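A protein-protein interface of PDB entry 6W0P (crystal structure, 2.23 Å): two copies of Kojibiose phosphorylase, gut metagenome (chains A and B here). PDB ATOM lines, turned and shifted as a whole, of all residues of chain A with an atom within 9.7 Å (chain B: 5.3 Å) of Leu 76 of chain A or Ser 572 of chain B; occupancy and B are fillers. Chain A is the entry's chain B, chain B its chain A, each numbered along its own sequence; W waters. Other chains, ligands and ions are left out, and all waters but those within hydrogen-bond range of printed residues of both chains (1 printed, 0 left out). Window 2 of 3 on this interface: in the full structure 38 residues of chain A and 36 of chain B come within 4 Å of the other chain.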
ATOM      1  N   PRO A  72      26.203 -35.979 -27.140  1.00  0.00           N
ATOM      2  CA  PRO A  72      24.998 -35.331 -27.641  1.00  0.00           C
ATOM      3  C   PRO A  72      24.640 -34.150 -26.731  1.00  0.00           C
ATOM      4  O   PRO A  72      25.032 -34.101 -25.574  1.00  0.00           O
ATOM      5  CB  PRO A  72      23.914 -36.430 -27.638  1.00  0.00           C
ATOM      6  CG  PRO A  72      24.504 -37.605 -26.835  1.00  0.00           C
ATOM      7  CD  PRO A  72      25.897 -37.201 -26.369  1.00  0.00           C
ATOM      8  N   SER A  73      23.919 -33.192 -27.297  1.00  0.00           N
ATOM      9  CA  SER A  73      23.301 -32.084 -26.538  1.00  0.00           C
ATOM     10  C   SER A  73      22.025 -31.638 -27.258  1.00  0.00           C
ATOM     11  O   SER A  73      22.056 -31.516 -28.521  1.00  0.00           O
ATOM     12  CB  SER A  73      24.281 -30.947 -26.352  1.00  0.00           C
ATOM     13  OG  SER A  73      23.731 -29.974 -25.484  1.00  0.00           O
ATOM     14  N   ALA A  74      20.966 -31.379 -26.481  1.00  0.00           N
ATOM     15  CA  ALA A  74      19.704 -30.751 -26.951  1.00  0.00           C
ATOM     16  C   ALA A  74      19.921 -29.265 -27.278  1.00  0.00           C
ATOM     17  O   ALA A  74      19.086 -28.709 -28.024  1.00  0.00           O
ATOM     18  CB  ALA A  74      18.627 -30.915 -25.904  1.00  0.00           C
ATOM     19  N   TYR A  75      21.004 -28.652 -26.780  1.00  0.00           N
ATOM     20  CA  TYR A  75      21.237 -27.178 -26.778  1.00  0.00           C
ATOM     21  C   TYR A  75      22.293 -26.744 -27.795  1.00  0.00           C
ATOM     22  O   TYR A  75      23.311 -27.416 -27.937  1.00  0.00           O
ATOM     23  CB  TYR A  75      21.691 -26.733 -25.391  1.00  0.00           C
ATOM     24  CG  TYR A  75      20.718 -27.122 -24.316  1.00  0.00           C
ATOM     25  CD1 TYR A  75      19.538 -26.413 -24.150  1.00  0.00           C
ATOM     26  CD2 TYR A  75      20.949 -28.227 -23.510  1.00  0.00           C
ATOM     27  CE1 TYR A  75      18.621 -26.765 -23.174  1.00  0.00           C
ATOM     28  CE2 TYR A  75      20.037 -28.598 -22.534  1.00  0.00           C
ATOM     29  CZ  TYR A  75      18.873 -27.862 -22.365  1.00  0.00           C
ATOM     30  OH  TYR A  75      17.966 -28.202 -21.407  1.00  0.00           O
ATOM     31  N   LEU A  76      22.092 -25.582 -28.415  1.00  0.00           N
ATOM     32  CA  LEU A  76      23.079 -24.987 -29.352  1.00  0.00           C
ATOM     33  C   LEU A  76      24.198 -24.284 -28.565  1.00  0.00           C
ATOM     34  O   LEU A  76      23.980 -23.916 -27.379  1.00  0.00           O
ATOM     35  CB  LEU A  76      22.370 -24.026 -30.307  1.00  0.00           C
ATOM     36  CG  LEU A  76      21.188 -24.622 -31.067  1.00  0.00           C
ATOM     37  CD1 LEU A  76      20.340 -23.516 -31.678  1.00  0.00           C
ATOM     38  CD2 LEU A  76      21.661 -25.594 -32.141  1.00  0.00           C
ATOM     39  N   GLY A  77      25.354 -24.112 -29.220  1.00  0.00           N
ATOM     40  CA  GLY A  77      26.546 -23.459 -28.669  1.00  0.00           C
ATOM     41  C   GLY A  77      27.368 -24.381 -27.799  1.00  0.00           C
ATOM     42  O   GLY A  77      28.416 -23.965 -27.366  1.00  0.00           O
ATOM     43  N   ILE A  78      26.961 -25.624 -27.589  1.00  0.00           N
ATOM     44  CA  ILE A  78      27.786 -26.567 -26.794  1.00  0.00           C
ATOM     45  C   ILE A  78      28.486 -27.546 -27.733  1.00  0.00           C
ATOM     46  O   ILE A  78      27.830 -28.119 -28.604  1.00  0.00           O
ATOM     47  CB  ILE A  78      26.946 -27.242 -25.702  1.00  0.00           C
ATOM     48  CG1 ILE A  78      26.354 -26.166 -24.776  1.00  0.00           C
ATOM     49  CG2 ILE A  78      27.780 -28.284 -24.955  1.00  0.00           C
ATOM     50  CD1 ILE A  78      25.338 -26.695 -23.793  1.00  0.00           C
ATOM     51  N   VAL A  79      29.781 -27.736 -27.503  1.00  0.00           N
ATOM     52  CA  VAL A  79      30.674 -28.581 -28.344  1.00  0.00           C
ATOM     53  C   VAL A  79      30.225 -30.032 -28.218  1.00  0.00           C
ATOM     54  O   VAL A  79      30.266 -30.582 -27.108  1.00  0.00           O
ATOM     55  CB  VAL A  79      32.144 -28.445 -27.911  1.00  0.00           C
ATOM     56  CG1 VAL A  79      33.031 -29.400 -28.697  1.00  0.00           C
ATOM     57  CG2 VAL A  79      32.650 -27.000 -28.031  1.00  0.00           C
ATOM     58  N   LYS A  80      29.848 -30.626 -29.334  1.00  0.00           N
ATOM     59  CA  LYS A  80      29.440 -32.040 -29.414  1.00  0.00           C
ATOM     60  C   LYS A  80      30.679 -32.884 -29.718  1.00  0.00           C
ATOM     61  O   LYS A  80      30.708 -34.059 -29.315  1.00  0.00           O
ATOM     62  CB  LYS A  80      28.357 -32.153 -30.483  1.00  0.00           C
ATOM     63  CG  LYS A  80      27.112 -31.312 -30.209  1.00  0.00           C
ATOM     64  CD  LYS A  80      25.945 -31.660 -31.119  1.00  0.00           C
ATOM     65  CE  LYS A  80      24.638 -31.040 -30.684  1.00  0.00           C
ATOM     66  NZ  LYS A  80      23.600 -31.224 -31.724  1.00  0.00           N
ATOM     67  N   ARG A 385      32.307 -19.582 -34.410  1.00  0.00           N
ATOM     68  CA  ARG A 385      32.105 -19.736 -32.936  1.00  0.00           C
ATOM     69  C   ARG A 385      31.213 -18.614 -32.390  1.00  0.00           C
ATOM     70  O   ARG A 385      30.372 -18.893 -31.519  1.00  0.00           O
ATOM     71  CB  ARG A 385      33.444 -19.713 -32.191  1.00  0.00           C
ATOM     72  CG  ARG A 385      33.316 -19.751 -30.672  1.00  0.00           C
ATOM     73  CD  ARG A 385      32.524 -20.968 -30.243  1.00  0.00           C
ATOM     74  NE  ARG A 385      32.387 -21.071 -28.811  1.00  0.00           N
ATOM     75  CZ  ARG A 385      31.492 -21.839 -28.207  1.00  0.00           C
ATOM     76  NH1 ARG A 385      30.658 -22.566 -28.921  1.00  0.00           N
ATOM     77  NH2 ARG A 385      31.411 -21.872 -26.890  1.00  0.00           N
ATOM     78  N   ALA A 386      31.408 -17.376 -32.844  1.00  0.00           N
ATOM     79  CA  ALA A 386      30.538 -16.236 -32.499  1.00  0.00           C
ATOM     80  C   ALA A 386      29.087 -16.564 -32.865  1.00  0.00           C
ATOM     81  O   ALA A 386      28.179 -16.314 -32.043  1.00  0.00           O
ATOM     82  CB  ALA A 386      31.032 -14.989 -33.194  1.00  0.00           C
ATOM     83  N   LYS A 387      28.857 -17.109 -34.060  1.00  0.00           N
ATOM     84  CA  LYS A 387      27.481 -17.499 -34.502  1.00  0.00           C
ATOM     85  C   LYS A 387      26.920 -18.584 -33.576  1.00  0.00           C
ATOM     86  O   LYS A 387      25.726 -18.513 -33.316  1.00  0.00           O
ATOM     87  CB  LYS A 387      27.443 -17.875 -35.985  1.00  0.00           C
ATOM     88  CG  LYS A 387      27.487 -16.648 -36.897  1.00  0.00           C
ATOM     89  CD  LYS A 387      27.454 -16.952 -38.384  1.00  0.00           C
ATOM     90  CE  LYS A 387      27.905 -15.760 -39.208  1.00  0.00           C
ATOM     91  NZ  LYS A 387      29.359 -15.821 -39.528  1.00  0.00           N
ATOM     92  N   GLU A 388      27.748 -19.516 -33.085  1.00  0.00           N
ATOM     93  CA  GLU A 388      27.305 -20.550 -32.107  1.00  0.00           C
ATOM     94  C   GLU A 388      26.858 -19.880 -30.786  1.00  0.00           C
ATOM     95  O   GLU A 388      26.029 -20.506 -30.070  1.00  0.00           O
ATOM     96  CB  GLU A 388      28.397 -21.598 -31.870  1.00  0.00           C
ATOM     97  CG  GLU A 388      28.664 -22.507 -33.072  1.00  0.00           C
ATOM     98  CD  GLU A 388      29.898 -23.396 -32.949  1.00  0.00           C
ATOM     99  OE1 GLU A 388      30.620 -23.301 -31.935  1.00  0.00           O
ATOM    100  OE2 GLU A 388      30.117 -24.206 -33.860  1.00  0.00           O
ATOM    101  N   LEU A 389      27.348 -18.665 -30.470  1.00  0.00           N
ATOM    102  CA  LEU A 389      26.936 -17.896 -29.253  1.00  0.00           C
ATOM    103  C   LEU A 389      25.949 -16.773 -29.613  1.00  0.00           C
ATOM    104  O   LEU A 389      25.875 -15.775 -28.855  1.00  0.00           O
ATOM    105  CB  LEU A 389      28.180 -17.362 -28.526  1.00  0.00           C
ATOM    106  CG  LEU A 389      29.215 -18.419 -28.117  1.00  0.00           C
ATOM    107  CD1 LEU A 389      30.412 -17.800 -27.404  1.00  0.00           C
ATOM    108  CD2 LEU A 389      28.566 -19.476 -27.240  1.00  0.00           C
ATOM    109  N   ASP A 390      25.200 -16.927 -30.698  1.00  0.00           N
ATOM    110  CA  ASP A 390      24.161 -15.966 -31.140  1.00  0.00           C
ATOM    111  C   ASP A 390      24.731 -14.541 -31.224  1.00  0.00           C
ATOM    112  O   ASP A 390      24.034 -13.615 -30.908  1.00  0.00           O
ATOM    113  CB  ASP A 390      22.955 -16.087 -30.199  1.00  0.00           C
ATOM    114  CG  ASP A 390      22.136 -17.335 -30.521  1.00  0.00           C
ATOM    115  OD1 ASP A 390      22.469 -18.031 -31.522  1.00  0.00           O
ATOM    116  OD2 ASP A 390      21.182 -17.605 -29.797  1.00  0.00           O
ATOM    117  N   TRP A 410      30.155 -25.615 -21.095  1.00  0.00           N
ATOM    118  CA  TRP A 410      29.468 -24.334 -21.378  1.00  0.00           C
ATOM    119  C   TRP A 410      29.838 -23.313 -20.285  1.00  0.00           C
ATOM    120  O   TRP A 410      29.947 -22.128 -20.622  1.00  0.00           O
ATOM    121  CB  TRP A 410      27.963 -24.539 -21.530  1.00  0.00           C
ATOM    122  CG  TRP A 410      27.295 -24.780 -20.214  1.00  0.00           C
ATOM    123  CD1 TRP A 410      27.054 -25.991 -19.637  1.00  0.00           C
ATOM    124  CD2 TRP A 410      26.871 -23.779 -19.273  1.00  0.00           C
ATOM    125  NE1 TRP A 410      26.469 -25.808 -18.416  1.00  0.00           N
ATOM    126  CE2 TRP A 410      26.352 -24.466 -18.159  1.00  0.00           C
ATOM    127  CE3 TRP A 410      26.869 -22.377 -19.263  1.00  0.00           C
ATOM    128  CZ2 TRP A 410      25.835 -23.799 -17.044  1.00  0.00           C
ATOM    129  CZ3 TRP A 410      26.356 -21.716 -18.168  1.00  0.00           C
ATOM    130  CH2 TRP A 410      25.838 -22.422 -17.077  1.00  0.00           C
ATOM    131  N   ALA A 413      33.154 -22.110 -21.880  1.00  0.00           N
ATOM    132  CA  ALA A 413      33.180 -21.860 -23.337  1.00  0.00           C
ATOM    133  C   ALA A 413      32.149 -20.790 -23.713  1.00  0.00           C
ATOM    134  O   ALA A 413      32.396 -20.072 -24.665  1.00  0.00           O
ATOM    135  CB  ALA A 413      32.947 -23.134 -24.099  1.00  0.00           C
ATOM    136  N   SER A 414      31.027 -20.721 -23.002  1.00  0.00           N
ATOM    137  CA  SER A 414      29.893 -19.805 -23.295  1.00  0.00           C
ATOM    138  C   SER A 414      30.018 -18.495 -22.503  1.00  0.00           C
ATOM    139  O   SER A 414      29.252 -17.569 -22.812  1.00  0.00           O
ATOM    140  CB  SER A 414      28.588 -20.464 -22.987  1.00  0.00           C
ATOM    141  OG  SER A 414      28.258 -21.422 -23.975  1.00  0.00           O
ATOM    142  N   PRO B 569      10.578 -23.914 -29.817  1.00  0.00           N
ATOM    143  CA  PRO B 569      10.893 -23.449 -28.462  1.00  0.00           C
ATOM    144  C   PRO B 569      12.317 -22.853 -28.411  1.00  0.00           C
ATOM    145  O   PRO B 569      13.092 -23.078 -29.346  1.00  0.00           O
ATOM    146  CB  PRO B 569      10.724 -24.715 -27.604  1.00  0.00           C
ATOM    147  CG  PRO B 569      11.037 -25.865 -28.556  1.00  0.00           C
ATOM    148  CD  PRO B 569      10.666 -25.381 -29.948  1.00  0.00           C
ATOM    149  N   ILE B 570      12.607 -22.070 -27.365  1.00  0.00           N
ATOM    150  CA  ILE B 570      13.857 -21.260 -27.208  1.00  0.00           C
ATOM    151  C   ILE B 570      15.083 -22.185 -27.229  1.00  0.00           C
ATOM    152  O   ILE B 570      16.053 -21.860 -27.942  1.00  0.00           O
ATOM    153  CB  ILE B 570      13.803 -20.424 -25.911  1.00  0.00           C
ATOM    154  CG1 ILE B 570      12.820 -19.252 -26.022  1.00  0.00           C
ATOM    155  CG2 ILE B 570      15.190 -19.947 -25.511  1.00  0.00           C
ATOM    156  CD1 ILE B 570      13.335 -18.069 -26.817  1.00  0.00           C
ATOM    157  N   TYR B 571      15.041 -23.287 -26.469  1.00  0.00           N
ATOM    158  CA  TYR B 571      16.208 -24.168 -26.196  1.00  0.00           C
ATOM    159  C   TYR B 571      16.709 -24.781 -27.515  1.00  0.00           C
ATOM    160  O   TYR B 571      17.920 -25.118 -27.596  1.00  0.00           O
ATOM    161  CB  TYR B 571      15.882 -25.194 -25.098  1.00  0.00           C
ATOM    162  CG  TYR B 571      14.854 -26.258 -25.418  1.00  0.00           C
ATOM    163  CD1 TYR B 571      15.160 -27.332 -26.250  1.00  0.00           C
ATOM    164  CD2 TYR B 571      13.585 -26.226 -24.848  1.00  0.00           C
ATOM    165  CE1 TYR B 571      14.230 -28.319 -26.538  1.00  0.00           C
ATOM    166  CE2 TYR B 571      12.644 -27.211 -25.121  1.00  0.00           C
ATOM    167  CZ  TYR B 571      12.967 -28.259 -25.971  1.00  0.00           C
ATOM    168  OH  TYR B 571      12.057 -29.239 -26.250  1.00  0.00           O
ATOM    169  N   SER B 572      15.829 -24.883 -28.519  1.00  0.00           N
ATOM    170  CA  SER B 572      16.104 -25.493 -29.845  1.00  0.00           C
ATOM    171  C   SER B 572      16.631 -24.455 -30.836  1.00  0.00           C
ATOM    172  O   SER B 572      17.157 -24.888 -31.885  1.00  0.00           O
ATOM    173  CB  SER B 572      14.876 -26.168 -30.404  1.00  0.00           C
ATOM    174  OG  SER B 572      14.424 -27.185 -29.525  1.00  0.00           O
ATOM    175  N   HIS B 573      16.470 -23.158 -30.563  1.00  0.00           N
ATOM    176  CA  HIS B 573      16.823 -22.094 -31.542  1.00  0.00           C
ATOM    177  C   HIS B 573      17.887 -21.128 -30.991  1.00  0.00           C
ATOM    178  O   HIS B 573      18.666 -20.642 -31.808  1.00  0.00           O
ATOM    179  CB  HIS B 573      15.548 -21.434 -32.115  1.00  0.00           C
ATOM    180  CG  HIS B 573      14.790 -22.348 -33.036  1.00  0.00           C
ATOM    181  ND1 HIS B 573      13.923 -23.332 -32.561  1.00  0.00           N
ATOM    182  CD2 HIS B 573      14.803 -22.479 -34.383  1.00  0.00           C
ATOM    183  CE1 HIS B 573      13.422 -24.004 -33.579  1.00  0.00           C
ATOM    184  NE2 HIS B 573      13.940 -23.494 -34.705  1.00  0.00           N
ATOM    185  N   TRP B 574      17.962 -20.899 -29.680  1.00  0.00           N
ATOM    186  CA  TRP B 574      18.922 -19.955 -29.036  1.00  0.00           C
ATOM    187  C   TRP B 574      20.131 -20.716 -28.483  1.00  0.00           C
ATOM    188  O   TRP B 574      19.949 -21.825 -28.004  1.00  0.00           O
ATOM    189  CB  TRP B 574      18.225 -19.146 -27.928  1.00  0.00           C
ATOM    190  CG  TRP B 574      17.315 -18.079 -28.446  1.00  0.00           C
ATOM    191  CD1 TRP B 574      16.802 -18.011 -29.704  1.00  0.00           C
ATOM    192  CD2 TRP B 574      16.785 -16.939 -27.738  1.00  0.00           C
ATOM    193  NE1 TRP B 574      16.015 -16.905 -29.839  1.00  0.00           N
ATOM    194  CE2 TRP B 574      15.970 -16.235 -28.652  1.00  0.00           C
ATOM    195  CE3 TRP B 574      16.936 -16.423 -26.441  1.00  0.00           C
ATOM    196  CZ2 TRP B 574      15.319 -15.052 -28.319  1.00  0.00           C
ATOM    197  CZ3 TRP B 574      16.289 -15.254 -26.115  1.00  0.00           C
ATOM    198  CH2 TRP B 574      15.483 -14.589 -27.036  1.00  0.00           C
ATOM    199  N   SER B 575      21.325 -20.134 -28.572  1.00  0.00           N
ATOM    200  CA  SER B 575      22.538 -20.612 -27.870  1.00  0.00           C
ATOM    201  C   SER B 575      22.187 -20.819 -26.393  1.00  0.00           C
ATOM    202  O   SER B 575      21.520 -19.985 -25.808  1.00  0.00           O
ATOM    203  CB  SER B 575      23.687 -19.660 -28.031  1.00  0.00           C
ATOM    204  OG  SER B 575      24.912 -20.279 -27.691  1.00  0.00           O
ATOM    205  N   TYR B 576      22.665 -21.892 -25.807  1.00  0.00           N
ATOM    206  CA  TYR B 576      22.356 -22.299 -24.421  1.00  0.00           C
ATOM    207  C   TYR B 576      22.347 -21.104 -23.449  1.00  0.00           C
ATOM    208  O   TYR B 576      21.361 -20.961 -22.718  1.00  0.00           O
ATOM    209  CB  TYR B 576      23.352 -23.339 -23.915  1.00  0.00           C
ATOM    210  CG  TYR B 576      23.005 -23.754 -22.508  1.00  0.00           C
ATOM    211  CD1 TYR B 576      21.751 -24.283 -22.243  1.00  0.00           C
ATOM    212  CD2 TYR B 576      23.847 -23.514 -21.441  1.00  0.00           C
ATOM    213  CE1 TYR B 576      21.378 -24.639 -20.964  1.00  0.00           C
ATOM    214  CE2 TYR B 576      23.482 -23.860 -20.145  1.00  0.00           C
ATOM    215  CZ  TYR B 576      22.255 -24.450 -19.915  1.00  0.00           C
ATOM    216  OH  TYR B 576      21.840 -24.823 -18.673  1.00  0.00           O
HETATM  217  O   HOH W   1      25.991 -20.668 -24.924  1.00  0.00           O
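Printed residues of chain B that touch a printed residue of chain A: Tyr 571, Ser 572, His 573, Trp 574, Ser 575 and Tyr 576. Hydrophobic or aromatic side chains of chain B within 4 Å of the printed part of chain A: Tyr 571, Trp 574 and Tyr 576. Of the 18 printed residues of chain A, 9 touch a printed residue of chain B. Hydrophobic or aromatic side chains of chain A that line the printed part of chain B: Tyr 75, Leu 76, Ile 78, Leu 389 and Trp 410. Among the printed residues, 14 pairs touch across the chains. Among the printed residues, no Asp or Glu carboxylate lies within 4 Å of a Lys or Arg side-chain nitrogen of the other chain.
The side-chain hydroxyl (OG) of Ser 575 of chain B sits at hydrogen-bond distance from the backbone carbonyl oxygen (O) of Glu 388 of chain A (2.6 Å). N of Ser 575 of chain B lies within hydrogen-bond range of OD2 of Asp 390 of chain A. The backbone NH of Tyr 576 of chain B sits at hydrogen-bond distance from the backbone carbonyl oxygen of Leu 76 of chain A (2.9 Å).
Of the printed residues of chain B, Leu 76 of chain A touches Ser 572, His 573, Ser 575 and Tyr 576. Of chain A, only Leu 76 comes within 4 Å of Ser 572 of chain B. No residue of chain A comes within 4 Å of Pro 569 of chain B. Tyr 571 of chain B touches just these residues of chain A: Ala 74 (3.8 Å) and Tyr 75 (3.7 Å). His 573 of chain B touches one residue of chain A. Of chain A, only Leu 76 (3.6 Å), Gly 77 (3.7 Å), Glu 388 (2.6 Å), Leu 389 (3.5 Å) and Asp 390 (2.8 Å) come within 4 Å of Ser 575 of chain B. Of the printed residues of chain B, Tyr 75 of chain A touches Tyr 571 (3.7 Å) and Tyr 576 (3.6 Å). Of the printed residues of chain A, Tyr 576 of chain B touches Tyr 75, Leu 76, Ile 78 and Trp 410. Of the printed residues of chain B, Ala 74 of chain A touches Tyr 571 (3.8 Å). The nearest printed residue of chain B that does not touch Leu 76 of chain A is Trp 574 of chain B (4.001 Å). The nearest residue of chain A that does not touch Ser 572 of chain B is Ala 74 of chain A (4.7 Å).
The side-chain carboxylate of Glu 388 of chain A is in salt-bridge range of the guanidinium group of Arg 385 of chain A, at 3.1 Å. A ring nitrogen (ND1) of His 573 of chain B is in hydrogen-bond range of the backbone carbonyl oxygen of Pro 569 of chain B (3.3 Å). The side-chain hydroxyl of Ser 73 of chain A lies close to the backbone NH of Tyr 75 of chain A, 3.3 Å away. O of Gly 77 of chain A lies within hydrogen-bond range of NH1 of Arg 385 of chain A (3.1 Å).
Ala 74 of chain A touches Tyr 571 of chain B (O to O, 3.8 Å). Tyr 75 of chain A touches Tyr 571 of chain B. Tyr 75 of chain A touches Tyr 576 of chain B (CD1 to CD1, 3.6 Å). Leu 76 of chain A touches Ser 572 of chain B (CD1 to O, 3.5 Å). CA of Ser 575 of chain B touches O of Leu 76 of chain A, at 3.6 Å. OG of Ser 575 of chain B touches CA of Gly 77 of chain A, 3.7 Å away. Tyr 576 of chain B touches Ile 78 of chain A. Ser 575 of chain B touches Leu 389 of chain A. Trp 574 of chain B touches Asp 390 of chain A (CA to OD2, 3.3 Å). CE2 of Tyr 576 of chain B touches CD2 of Trp 410 of chain A, 3.5 Å away.
Water W1 lies within hydrogen-bond range of OG of Ser 414 of chain A (2.6 Å) and OG of Ser 575 of chain B (3.0 Å).
No position is printed for both chains. Of the 14 pairs that touch across the chains among the printed residues, none has its exchanged pair printed and touching as well.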
